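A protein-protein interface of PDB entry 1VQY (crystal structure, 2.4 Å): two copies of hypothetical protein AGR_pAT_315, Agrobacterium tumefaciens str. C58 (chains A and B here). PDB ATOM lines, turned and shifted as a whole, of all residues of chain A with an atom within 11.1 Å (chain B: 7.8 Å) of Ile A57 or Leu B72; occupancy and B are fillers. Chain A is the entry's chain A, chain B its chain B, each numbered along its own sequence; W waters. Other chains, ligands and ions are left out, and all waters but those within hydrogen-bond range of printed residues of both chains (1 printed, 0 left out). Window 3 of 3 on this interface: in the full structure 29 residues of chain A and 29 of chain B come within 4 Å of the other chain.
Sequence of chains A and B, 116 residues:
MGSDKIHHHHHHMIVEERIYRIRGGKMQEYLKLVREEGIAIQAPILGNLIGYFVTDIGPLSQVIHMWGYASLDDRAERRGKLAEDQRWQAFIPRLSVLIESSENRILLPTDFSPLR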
ATOM      1  N   PHE A  53      -4.625 -23.091  25.903  1.00  0.00           N
ATOM      2  CA  PHE A  53      -3.984 -22.936  24.586  1.00  0.00           C
ATOM      3  C   PHE A  53      -3.242 -21.615  24.402  1.00  0.00           C
ATOM      4  O   PHE A  53      -3.605 -20.593  24.992  1.00  0.00           O
ATOM      5  CB  PHE A  53      -5.023 -23.033  23.465  1.00  0.00           C
ATOM      6  CG  PHE A  53      -6.027 -24.170  23.617  1.00  0.00           C
ATOM      7  CD1 PHE A  53      -5.785 -25.414  23.069  1.00  0.00           C
ATOM      8  CD2 PHE A  53      -7.238 -23.964  24.274  1.00  0.00           C
ATOM      9  CE1 PHE A  53      -6.724 -26.436  23.177  1.00  0.00           C
ATOM     10  CE2 PHE A  53      -8.199 -24.979  24.375  1.00  0.00           C
ATOM     11  CZ  PHE A  53      -7.941 -26.215  23.829  1.00  0.00           C
ATOM     12  N   VAL A  54      -2.213 -21.655  23.557  1.00  0.00           N
ATOM     13  CA  VAL A  54      -1.469 -20.468  23.122  1.00  0.00           C
ATOM     14  C   VAL A  54      -1.644 -20.382  21.622  1.00  0.00           C
ATOM     15  O   VAL A  54      -1.362 -21.351  20.922  1.00  0.00           O
ATOM     16  CB  VAL A  54       0.025 -20.607  23.420  1.00  0.00           C
ATOM     17  CG1 VAL A  54       0.812 -19.332  22.984  1.00  0.00           C
ATOM     18  CG2 VAL A  54       0.228 -20.934  24.883  1.00  0.00           C
ATOM     19  N   THR A  55      -2.128 -19.244  21.127  1.00  0.00           N
ATOM     20  CA  THR A  55      -2.401 -19.083  19.708  1.00  0.00           C
ATOM     21  C   THR A  55      -1.111 -19.048  18.897  1.00  0.00           C
ATOM     22  O   THR A  55      -0.183 -18.314  19.230  1.00  0.00           O
ATOM     23  CB  THR A  55      -3.178 -17.789  19.457  1.00  0.00           C
ATOM     24  OG1 THR A  55      -4.359 -17.777  20.260  1.00  0.00           O
ATOM     25  CG2 THR A  55      -3.584 -17.665  17.986  1.00  0.00           C
ATOM     26  N   ASP A  56      -1.071 -19.853  17.840  1.00  0.00           N
ATOM     27  CA  ASP A  56       0.045 -19.879  16.866  1.00  0.00           C
ATOM     28  C   ASP A  56      -0.279 -19.012  15.640  1.00  0.00           C
ATOM     29  O   ASP A  56       0.613 -18.360  15.083  1.00  0.00           O
ATOM     30  CB  ASP A  56       0.342 -21.337  16.429  1.00  0.00           C
ATOM     31  CG  ASP A  56       1.472 -21.444  15.415  1.00  0.00           C
ATOM     32  OD1 ASP A  56       2.557 -20.868  15.629  1.00  0.00           O
ATOM     33  OD2 ASP A  56       1.284 -22.124  14.385  1.00  0.00           O
ATOM     34  N   ILE A  57      -1.548 -19.018  15.217  1.00  0.00           N
ATOM     35  CA  ILE A  57      -1.970 -18.237  14.054  1.00  0.00           C
ATOM     36  C   ILE A  57      -3.318 -17.549  14.305  1.00  0.00           C
ATOM     37  O   ILE A  57      -4.333 -18.193  14.602  1.00  0.00           O
ATOM     38  CB  ILE A  57      -2.052 -19.101  12.780  1.00  0.00           C
ATOM     39  CG1 ILE A  57      -0.783 -19.947  12.604  1.00  0.00           C
ATOM     40  CG2 ILE A  57      -2.283 -18.216  11.544  1.00  0.00           C
ATOM     41  CD1 ILE A  57      -0.881 -20.982  11.506  1.00  0.00           C
ATOM     42  N   GLY A  58      -3.307 -16.235  14.152  1.00  0.00           N
ATOM     43  CA  GLY A  58      -4.391 -15.374  14.585  1.00  0.00           C
ATOM     44  C   GLY A  58      -3.835 -14.275  15.497  1.00  0.00           C
ATOM     45  O   GLY A  58      -2.731 -13.756  15.268  1.00  0.00           O
ATOM     46  N   PRO A  59      -4.606 -13.887  16.515  1.00  0.00           N
ATOM     47  CA  PRO A  59      -4.058 -12.937  17.468  1.00  0.00           C
ATOM     48  C   PRO A  59      -2.924 -13.567  18.246  1.00  0.00           C
ATOM     49  O   PRO A  59      -3.077 -14.641  18.792  1.00  0.00           O
ATOM     50  CB  PRO A  59      -5.254 -12.597  18.379  1.00  0.00           C
ATOM     51  CG  PRO A  59      -6.490 -13.033  17.587  1.00  0.00           C
ATOM     52  CD  PRO A  59      -6.014 -14.225  16.795  1.00  0.00           C
ATOM     53  N   LEU A  60      -1.794 -12.882  18.303  1.00  0.00           N
ATOM     54  CA  LEU A  60      -0.588 -13.458  18.872  1.00  0.00           C
ATOM     55  C   LEU A  60      -0.313 -12.910  20.284  1.00  0.00           C
ATOM     56  O   LEU A  60      -0.915 -11.920  20.726  1.00  0.00           O
ATOM     57  CB  LEU A  60       0.591 -13.249  17.913  1.00  0.00           C
ATOM     58  CG  LEU A  60       0.492 -14.017  16.592  1.00  0.00           C
ATOM     59  CD1 LEU A  60       1.588 -13.638  15.664  1.00  0.00           C
ATOM     60  CD2 LEU A  60       0.477 -15.528  16.816  1.00  0.00           C
ATOM     61  N   SER A  61       0.566 -13.604  20.992  1.00  0.00           N
ATOM     62  CA  SER A  61       0.696 -13.459  22.420  1.00  0.00           C
ATOM     63  C   SER A  61      -0.672 -13.573  23.108  1.00  0.00           C
ATOM     64  O   SER A  61      -1.026 -12.776  23.992  1.00  0.00           O
ATOM     65  CB  SER A  61       1.384 -12.148  22.762  1.00  0.00           C
ATOM     66  OG  SER A  61       1.868 -12.197  24.087  1.00  0.00           O
ATOM     67  N   GLN A  62      -1.424 -14.595  22.714  1.00  0.00           N
ATOM     68  CA  GLN A  62      -2.783 -14.815  23.213  1.00  0.00           C
ATOM     69  C   GLN A  62      -2.889 -16.213  23.867  1.00  0.00           C
ATOM     70  O   GLN A  62      -2.449 -17.199  23.276  1.00  0.00           O
ATOM     71  CB  GLN A  62      -3.769 -14.677  22.042  1.00  0.00           C
ATOM     72  CG  GLN A  62      -5.220 -15.039  22.383  1.00  0.00           C
ATOM     73  CD  GLN A  62      -6.188 -14.816  21.226  1.00  0.00           C
ATOM     74  OE1 GLN A  62      -6.335 -15.678  20.352  1.00  0.00           O
ATOM     75  NE2 GLN A  62      -6.878 -13.663  21.231  1.00  0.00           N
ATOM     76  N   VAL A  63      -3.421 -16.273  25.094  1.00  0.00           N
ATOM     77  CA  VAL A  63      -3.824 -17.542  25.728  1.00  0.00           C
ATOM     78  C   VAL A  63      -5.342 -17.654  25.831  1.00  0.00           C
ATOM     79  O   VAL A  63      -6.029 -16.699  26.162  1.00  0.00           O
ATOM     80  CB  VAL A  63      -3.247 -17.800  27.169  1.00  0.00           C
ATOM     81  CG1 VAL A  63      -1.794 -18.077  27.119  1.00  0.00           C
ATOM     82  CG2 VAL A  63      -3.516 -16.663  28.098  1.00  0.00           C
ATOM     83  N   ILE A  64      -5.847 -18.854  25.577  1.00  0.00           N
ATOM     84  CA  ILE A  64      -7.247 -19.145  25.724  1.00  0.00           C
ATOM     85  C   ILE A  64      -7.360 -20.321  26.685  1.00  0.00           C
ATOM     86  O   ILE A  64      -6.671 -21.323  26.501  1.00  0.00           O
ATOM     87  CB  ILE A  64      -7.834 -19.482  24.354  1.00  0.00           C
ATOM     88  CG1 ILE A  64      -7.877 -18.216  23.493  1.00  0.00           C
ATOM     89  CG2 ILE A  64      -9.217 -20.113  24.470  1.00  0.00           C
ATOM     90  CD1 ILE A  64      -7.799 -18.500  22.034  1.00  0.00           C
ATOM     91  N   ILE B  14      -3.034 -30.043  17.082  1.00  0.00           N
ATOM     92  CA  ILE B  14      -3.380 -28.639  17.038  1.00  0.00           C
ATOM     93  C   ILE B  14      -4.884 -28.534  17.051  1.00  0.00           C
ATOM     94  O   ILE B  14      -5.579 -29.501  16.742  1.00  0.00           O
ATOM     95  CB  ILE B  14      -2.712 -27.916  15.845  1.00  0.00           C
ATOM     96  CG1 ILE B  14      -3.177 -28.472  14.497  1.00  0.00           C
ATOM     97  CG2 ILE B  14      -1.187 -28.068  15.948  1.00  0.00           C
ATOM     98  CD1 ILE B  14      -4.403 -27.809  13.945  1.00  0.00           C
ATOM     99  N   VAL B  15      -5.377 -27.372  17.463  1.00  0.00           N
ATOM    100  CA  VAL B  15      -6.806 -27.108  17.565  1.00  0.00           C
ATOM    101  C   VAL B  15      -7.174 -25.859  16.742  1.00  0.00           C
ATOM    102  O   VAL B  15      -6.579 -24.802  16.906  1.00  0.00           O
ATOM    103  CB  VAL B  15      -7.210 -26.907  19.050  1.00  0.00           C
ATOM    104  CG1 VAL B  15      -8.624 -26.328  19.177  1.00  0.00           C
ATOM    105  CG2 VAL B  15      -7.094 -28.226  19.809  1.00  0.00           C
ATOM    106  N   GLU B  16      -8.157 -25.987  15.860  1.00  0.00           N
ATOM    107  CA  GLU B  16      -8.660 -24.840  15.133  1.00  0.00           C
ATOM    108  C   GLU B  16      -9.950 -24.332  15.761  1.00  0.00           C
ATOM    109  O   GLU B  16     -10.895 -25.087  15.951  1.00  0.00           O
ATOM    110  CB  GLU B  16      -8.919 -25.172  13.671  1.00  0.00           C
ATOM    111  CG  GLU B  16      -9.669 -24.043  12.940  1.00  0.00           C
ATOM    112  CD  GLU B  16      -9.932 -24.334  11.483  1.00  0.00           C
ATOM    113  OE1 GLU B  16      -9.988 -25.518  11.090  1.00  0.00           O
ATOM    114  OE2 GLU B  16     -10.071 -23.359  10.732  1.00  0.00           O
ATOM    115  N   GLU B  17      -9.974 -23.034  16.053  1.00  0.00           N
ATOM    116  CA  GLU B  17     -11.179 -22.341  16.521  1.00  0.00           C
ATOM    117  C   GLU B  17     -11.769 -21.506  15.390  1.00  0.00           C
ATOM    118  O   GLU B  17     -11.102 -20.641  14.873  1.00  0.00           O
ATOM    119  CB  GLU B  17     -10.843 -21.438  17.712  1.00  0.00           C
ATOM    120  CG  GLU B  17     -12.055 -20.831  18.408  1.00  0.00           C
ATOM    121  CD  GLU B  17     -11.681 -20.169  19.742  1.00  0.00           C
ATOM    122  OE1 GLU B  17     -10.484 -19.874  19.933  1.00  0.00           O
ATOM    123  OE2 GLU B  17     -12.575 -19.959  20.597  1.00  0.00           O
ATOM    124  N   TYR B  69      -6.728 -31.503  15.007  1.00  0.00           N
ATOM    125  CA  TYR B  69      -5.951 -32.063  13.901  1.00  0.00           C
ATOM    126  C   TYR B  69      -4.552 -32.471  14.356  1.00  0.00           C
ATOM    127  O   TYR B  69      -4.047 -31.988  15.379  1.00  0.00           O
ATOM    128  CB  TYR B  69      -5.814 -31.069  12.751  1.00  0.00           C
ATOM    129  CG  TYR B  69      -7.088 -30.689  12.057  1.00  0.00           C
ATOM    130  CD1 TYR B  69      -7.675 -31.533  11.116  1.00  0.00           C
ATOM    131  CD2 TYR B  69      -7.695 -29.473  12.308  1.00  0.00           C
ATOM    132  CE1 TYR B  69      -8.844 -31.180  10.458  1.00  0.00           C
ATOM    133  CE2 TYR B  69      -8.863 -29.109  11.663  1.00  0.00           C
ATOM    134  CZ  TYR B  69      -9.432 -29.963  10.734  1.00  0.00           C
ATOM    135  OH  TYR B  69     -10.599 -29.583  10.099  1.00  0.00           O
ATOM    136  N   ALA B  70      -3.927 -33.359  13.592  1.00  0.00           N
ATOM    137  CA  ALA B  70      -2.594 -33.856  13.939  1.00  0.00           C
ATOM    138  C   ALA B  70      -1.505 -32.868  13.526  1.00  0.00           C
ATOM    139  O   ALA B  70      -0.494 -32.713  14.224  1.00  0.00           O
ATOM    140  CB  ALA B  70      -2.346 -35.229  13.298  1.00  0.00           C
ATOM    141  N   SER B  71      -1.718 -32.225  12.380  1.00  0.00           N
ATOM    142  CA  SER B  71      -0.816 -31.200  11.853  1.00  0.00           C
ATOM    143  C   SER B  71      -1.616 -30.230  10.985  1.00  0.00           C
ATOM    144  O   SER B  71      -2.813 -30.458  10.733  1.00  0.00           O
ATOM    145  CB  SER B  71       0.290 -31.841  11.026  1.00  0.00           C
ATOM    146  OG  SER B  71      -0.231 -32.375   9.819  1.00  0.00           O
ATOM    147  N   LEU B  72      -0.978 -29.156  10.526  1.00  0.00           N
ATOM    148  CA  LEU B  72      -1.672 -28.201   9.664  1.00  0.00           C
ATOM    149  C   LEU B  72      -1.816 -28.707   8.227  1.00  0.00           C
ATOM    150  O   LEU B  72      -2.752 -28.303   7.533  1.00  0.00           O
ATOM    151  CB  LEU B  72      -1.014 -26.821   9.701  1.00  0.00           C
ATOM    152  CG  LEU B  72      -1.304 -25.984  10.968  1.00  0.00           C
ATOM    153  CD1 LEU B  72      -0.491 -24.708  10.968  1.00  0.00           C
ATOM    154  CD2 LEU B  72      -2.786 -25.650  11.128  1.00  0.00           C
ATOM    155  N   ASP B  73      -0.908 -29.595   7.797  1.00  0.00           N
ATOM    156  CA  ASP B  73      -1.045 -30.289   6.501  1.00  0.00           C
ATOM    157  C   ASP B  73      -2.137 -31.333   6.534  1.00  0.00           C
ATOM    158  O   ASP B  73      -2.865 -31.494   5.557  1.00  0.00           O
ATOM    159  CB  ASP B  73       0.264 -30.955   6.060  1.00  0.00           C
ATOM    160  CG  ASP B  73       1.301 -29.941   5.583  1.00  0.00           C
ATOM    161  OD1 ASP B  73       1.142 -28.724   5.890  1.00  0.00           O
ATOM    162  OD2 ASP B  73       2.273 -30.372   4.914  1.00  0.00           O
ATOM    163  N   ASP B  74      -2.241 -32.057   7.644  1.00  0.00           N
ATOM    164  CA  ASP B  74      -3.387 -32.930   7.853  1.00  0.00           C
ATOM    165  C   ASP B  74      -4.667 -32.120   7.770  1.00  0.00           C
ATOM    166  O   ASP B  74      -5.629 -32.556   7.124  1.00  0.00           O
ATOM    167  CB  ASP B  74      -3.331 -33.618   9.213  1.00  0.00           C
ATOM    168  CG  ASP B  74      -4.422 -34.670   9.382  1.00  0.00           C
ATOM    169  OD1 ASP B  74      -4.450 -35.585   8.538  1.00  0.00           O
ATOM    170  OD2 ASP B  74      -5.225 -34.580  10.357  1.00  0.00           O
ATOM    171  N   ARG B  75      -4.692 -30.956   8.424  1.00  0.00           N
ATOM    172  CA  ARG B  75      -5.868 -30.092   8.344  1.00  0.00           C
ATOM    173  C   ARG B  75      -6.185 -29.754   6.879  1.00  0.00           C
ATOM    174  O   ARG B  75      -7.333 -29.870   6.443  1.00  0.00           O
ATOM    175  CB  ARG B  75      -5.704 -28.803   9.153  1.00  0.00           C
ATOM    176  CG  ARG B  75      -6.980 -27.957   9.113  1.00  0.00           C
ATOM    177  CD  ARG B  75      -6.877 -26.610   9.831  1.00  0.00           C
ATOM    178  NE  ARG B  75      -6.495 -25.623   8.838  1.00  0.00           N
ATOM    179  CZ  ARG B  75      -7.290 -24.732   8.263  1.00  0.00           C
ATOM    180  NH1 ARG B  75      -8.534 -24.535   8.639  1.00  0.00           N
ATOM    181  NH2 ARG B  75      -6.776 -23.962   7.327  1.00  0.00           N
ATOM    182  N   ALA B  76      -5.146 -29.357   6.137  1.00  0.00           N
ATOM    183  CA  ALA B  76      -5.282 -28.925   4.744  1.00  0.00           C
ATOM    184  C   ALA B  76      -5.785 -30.067   3.879  1.00  0.00           C
ATOM    185  O   ALA B  76      -6.657 -29.868   3.012  1.00  0.00           O
ATOM    186  CB  ALA B  76      -3.951 -28.414   4.217  1.00  0.00           C
ATOM    187  N   GLU B  77      -5.235 -31.255   4.121  1.00  0.00           N
ATOM    188  CA  GLU B  77      -5.682 -32.452   3.444  1.00  0.00           C
ATOM    189  C   GLU B  77      -7.177 -32.713   3.656  1.00  0.00           C
ATOM    190  O   GLU B  77      -7.910 -32.964   2.703  1.00  0.00           O
ATOM    191  CB  GLU B  77      -4.885 -33.654   3.928  1.00  0.00           C
ATOM    192  CG  GLU B  77      -5.309 -34.949   3.261  1.00  0.00           C
ATOM    193  CD  GLU B  77      -4.247 -36.034   3.331  1.00  0.00           C
ATOM    194  OE1 GLU B  77      -3.345 -35.939   4.211  1.00  0.00           O
ATOM    195  OE2 GLU B  77      -4.323 -36.979   2.498  1.00  0.00           O
ATOM    196  N   ARG B  78      -7.607 -32.644   4.914  1.00  0.00           N
ATOM    197  CA  ARG B  78      -8.978 -32.987   5.305  1.00  0.00           C
ATOM    198  C   ARG B  78      -9.982 -31.898   4.910  1.00  0.00           C
ATOM    199  O   ARG B  78     -11.121 -32.185   4.508  1.00  0.00           O
ATOM    200  CB  ARG B  78      -9.027 -33.260   6.801  1.00  0.00           C
ATOM    201  CG  ARG B  78      -8.430 -34.591   7.176  1.00  0.00           C
ATOM    202  CD  ARG B  78      -8.015 -34.625   8.638  1.00  0.00           C
ATOM    203  NE  ARG B  78      -7.597 -35.960   9.071  1.00  0.00           N
ATOM    204  CZ  ARG B  78      -8.432 -36.942   9.390  1.00  0.00           C
ATOM    205  NH1 ARG B  78      -9.744 -36.767   9.318  1.00  0.00           N
ATOM    206  NH2 ARG B  78      -7.955 -38.115   9.769  1.00  0.00           N
ATOM    207  N   ARG B  79      -9.554 -30.646   4.995  1.00  0.00           N
ATOM    208  CA  ARG B  79     -10.409 -29.557   4.569  1.00  0.00           C
ATOM    209  C   ARG B  79     -10.585 -29.580   3.055  1.00  0.00           C
ATOM    210  O   ARG B  79     -11.646 -29.203   2.545  1.00  0.00           O
ATOM    211  CB  ARG B  79      -9.892 -28.213   5.085  1.00  0.00           C
ATOM    212  CG  ARG B  79     -10.193 -28.009   6.565  1.00  0.00           C
ATOM    213  CD  ARG B  79     -10.059 -26.565   7.009  1.00  0.00           C
ATOM    214  NE  ARG B  79     -11.031 -25.668   6.357  1.00  0.00           N
ATOM    215  CZ  ARG B  79     -12.307 -25.510   6.724  1.00  0.00           C
ATOM    216  NH1 ARG B  79     -12.828 -26.191   7.747  1.00  0.00           N
ATOM    217  NH2 ARG B  79     -13.075 -24.671   6.045  1.00  0.00           N
ATOM    218  N   ASN B 104     -10.894 -17.548  11.970  1.00  0.00           N
ATOM    219  CA  ASN B 104     -10.374 -18.739  12.634  1.00  0.00           C
ATOM    220  C   ASN B 104      -8.994 -18.483  13.171  1.00  0.00           C
ATOM    221  O   ASN B 104      -8.392 -17.444  12.894  1.00  0.00           O
ATOM    222  CB  ASN B 104     -10.329 -19.938  11.698  1.00  0.00           C
ATOM    223  CG  ASN B 104      -9.423 -19.718  10.510  1.00  0.00           C
ATOM    224  OD1 ASN B 104      -9.056 -18.595  10.216  1.00  0.00           O
ATOM    225  ND2 ASN B 104      -9.081 -20.788   9.808  1.00  0.00           N
ATOM    226  N   ARG B 105      -8.505 -19.433  13.946  1.00  0.00           N
ATOM    227  CA  ARG B 105      -7.174 -19.349  14.484  1.00  0.00           C
ATOM    228  C   ARG B 105      -6.682 -20.711  14.901  1.00  0.00           C
ATOM    229  O   ARG B 105      -7.478 -21.607  15.162  1.00  0.00           O
ATOM    230  CB  ARG B 105      -7.129 -18.390  15.669  1.00  0.00           C
ATOM    231  CG  ARG B 105      -8.161 -18.644  16.754  1.00  0.00           C
ATOM    232  CD  ARG B 105      -8.160 -17.474  17.700  1.00  0.00           C
ATOM    233  NE  ARG B 105      -8.963 -17.692  18.898  1.00  0.00           N
ATOM    234  CZ  ARG B 105      -9.691 -16.756  19.498  1.00  0.00           C
ATOM    235  NH1 ARG B 105      -9.744 -15.519  18.993  1.00  0.00           N
ATOM    236  NH2 ARG B 105     -10.393 -17.058  20.586  1.00  0.00           N
ATOM    237  N   ILE B 106      -5.366 -20.857  14.961  1.00  0.00           N
ATOM    238  CA  ILE B 106      -4.772 -22.120  15.341  1.00  0.00           C
ATOM    239  C   ILE B 106      -4.228 -21.990  16.761  1.00  0.00           C
ATOM    240  O   ILE B 106      -3.410 -21.107  17.055  1.00  0.00           O
ATOM    241  CB  ILE B 106      -3.661 -22.549  14.348  1.00  0.00           C
ATOM    242  CG1 ILE B 106      -4.245 -22.722  12.924  1.00  0.00           C
ATOM    243  CG2 ILE B 106      -2.946 -23.826  14.826  1.00  0.00           C
ATOM    244  CD1 ILE B 106      -5.277 -23.834  12.736  1.00  0.00           C
ATOM    245  N   LEU B 107      -4.707 -22.887  17.623  1.00  0.00           N
ATOM    246  CA  LEU B 107      -4.327 -22.952  19.018  1.00  0.00           C
ATOM    247  C   LEU B 107      -3.447 -24.182  19.298  1.00  0.00           C
ATOM    248  O   LEU B 107      -3.730 -25.299  18.849  1.00  0.00           O
ATOM    249  CB  LEU B 107      -5.588 -23.014  19.868  1.00  0.00           C
ATOM    250  CG  LEU B 107      -6.714 -22.028  19.542  1.00  0.00           C
ATOM    251  CD1 LEU B 107      -7.911 -22.238  20.449  1.00  0.00           C
ATOM    252  CD2 LEU B 107      -6.234 -20.613  19.661  1.00  0.00           C
ATOM    253  N   LEU B 108      -2.366 -23.957  20.036  1.00  0.00           N
ATOM    254  CA  LEU B 108      -1.486 -25.017  20.486  1.00  0.00           C
ATOM    255  C   LEU B 108      -1.751 -25.281  21.961  1.00  0.00           C
ATOM    256  O   LEU B 108      -1.518 -24.407  22.782  1.00  0.00           O
ATOM    257  CB  LEU B 108      -0.032 -24.597  20.305  1.00  0.00           C
ATOM    258  CG  LEU B 108       0.380 -24.142  18.900  1.00  0.00           C
ATOM    259  CD1 LEU B 108       1.894 -23.966  18.833  1.00  0.00           C
ATOM    260  CD2 LEU B 108      -0.091 -25.124  17.799  1.00  0.00           C
HETATM  261  O   HOH W   1      -9.276 -12.296  19.820  1.00  0.00           O
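Leu B108 touches Phe A53 (O to CA, 3.4 Å). Val A54 touches Leu B107 (O to CA, 3.9 Å). Thr A55 touches Ile B106. Leu B107 touches Thr A55. Asp A56 touches Leu B108 (CB to CG, 3.7 Å). Ile A57 touches Leu B72. Pro A59 touches Arg B105. Gln A62 touches Arg B105 (OE1 to NE, 3.6 Å). Glu B17 touches Ile A64 (OE1 to CD1, 3.7 Å). Arg B105 touches Ile A64.
Water W1 bridges NE2 of Gln A62 (3.1 Å) and NH1 of Arg B105 (3.4 Å).
No position is printed for both chains. Of the 17 pairs that touch across the chains among the printed residues, none has its exchanged pair printed and touching as well.
Of the 20 printed residues of chain B, 7 touch a printed residue of chain A. Hydrophobic or aromatic side chains of chain B that line the printed part of chain A: Val B15, Leu B72, Leu B107 and Leu B108. Among the printed residues, 17 pairs touch across the chains. Among the printed residues, no Asp or Glu carboxylate lies within 4 Å of a Lys or Arg side-chain nitrogen of the other chain.
N of Phe A53 sits at hydrogen-bond distance from O of Ile A64, at 2.8 Å. OG1 of Thr A55 lies within hydrogen-bond range of OE1 of Gln A62, at 2.9 Å. The backbone carbonyl oxygen of Val B15 is in hydrogen-bond range of the backbone NH of Leu B107 (2.8 Å). The side-chain carboxylate of Glu B17 is in salt-bridge range of the guanidinium group of Arg B105 (2.9 Å).
The backbone carbonyl oxygen (O) of Val A54 sits at hydrogen-bond distance from the backbone NH (N) of Leu B108 (2.9 Å). The backbone carbonyl oxygen (O) of Ile B106 sits at hydrogen-bond distance from the backbone NH (N) of Asp A56 (2.8 Å). O of Ile A57 lies within hydrogen-bond range of N of Ile B106, 2.9 Å away.
Ile A57 touches just these residues of chain B: Leu B72, Arg B105 and Ile B106. Of the printed residues of chain A, Leu B72 touches Ile A57 (3.8 Å). No residue of chain A comes within 4 Å of Ala B70. Ser B71 touches none of the printed residues of chain A. No residue of chain A comes within 4 Å of Asp B73. No residue of chain A comes within 4 Å of Ala B76. Printed residues of chain A within 4 Å of Ile B106: Thr A55 (3.5 Å), Asp A56 (2.8 Å) and Ile A57 (2.9 Å). Of the printed residues of chain A, Glu B17 touches Ile A64 (3.7 Å). Printed residues of chain B within 4 Å of Gln A62: Arg B105. Of the printed residues of chain B, Thr A55 touches Ile B106 and Leu B107. Of the printed residues of chain A, Val B15 touches Phe A53 (3.8 Å). Printed residues of chain B within 4 Å of Pro A59: Arg B105 (3.998 Å). Arg B78 touches none of the printed residues of chain A. Asp B74 touches none of the printed residues of chain A. The nearest residue of chain A that does not touch Leu B72 is Asp A56 (4.6 Å).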
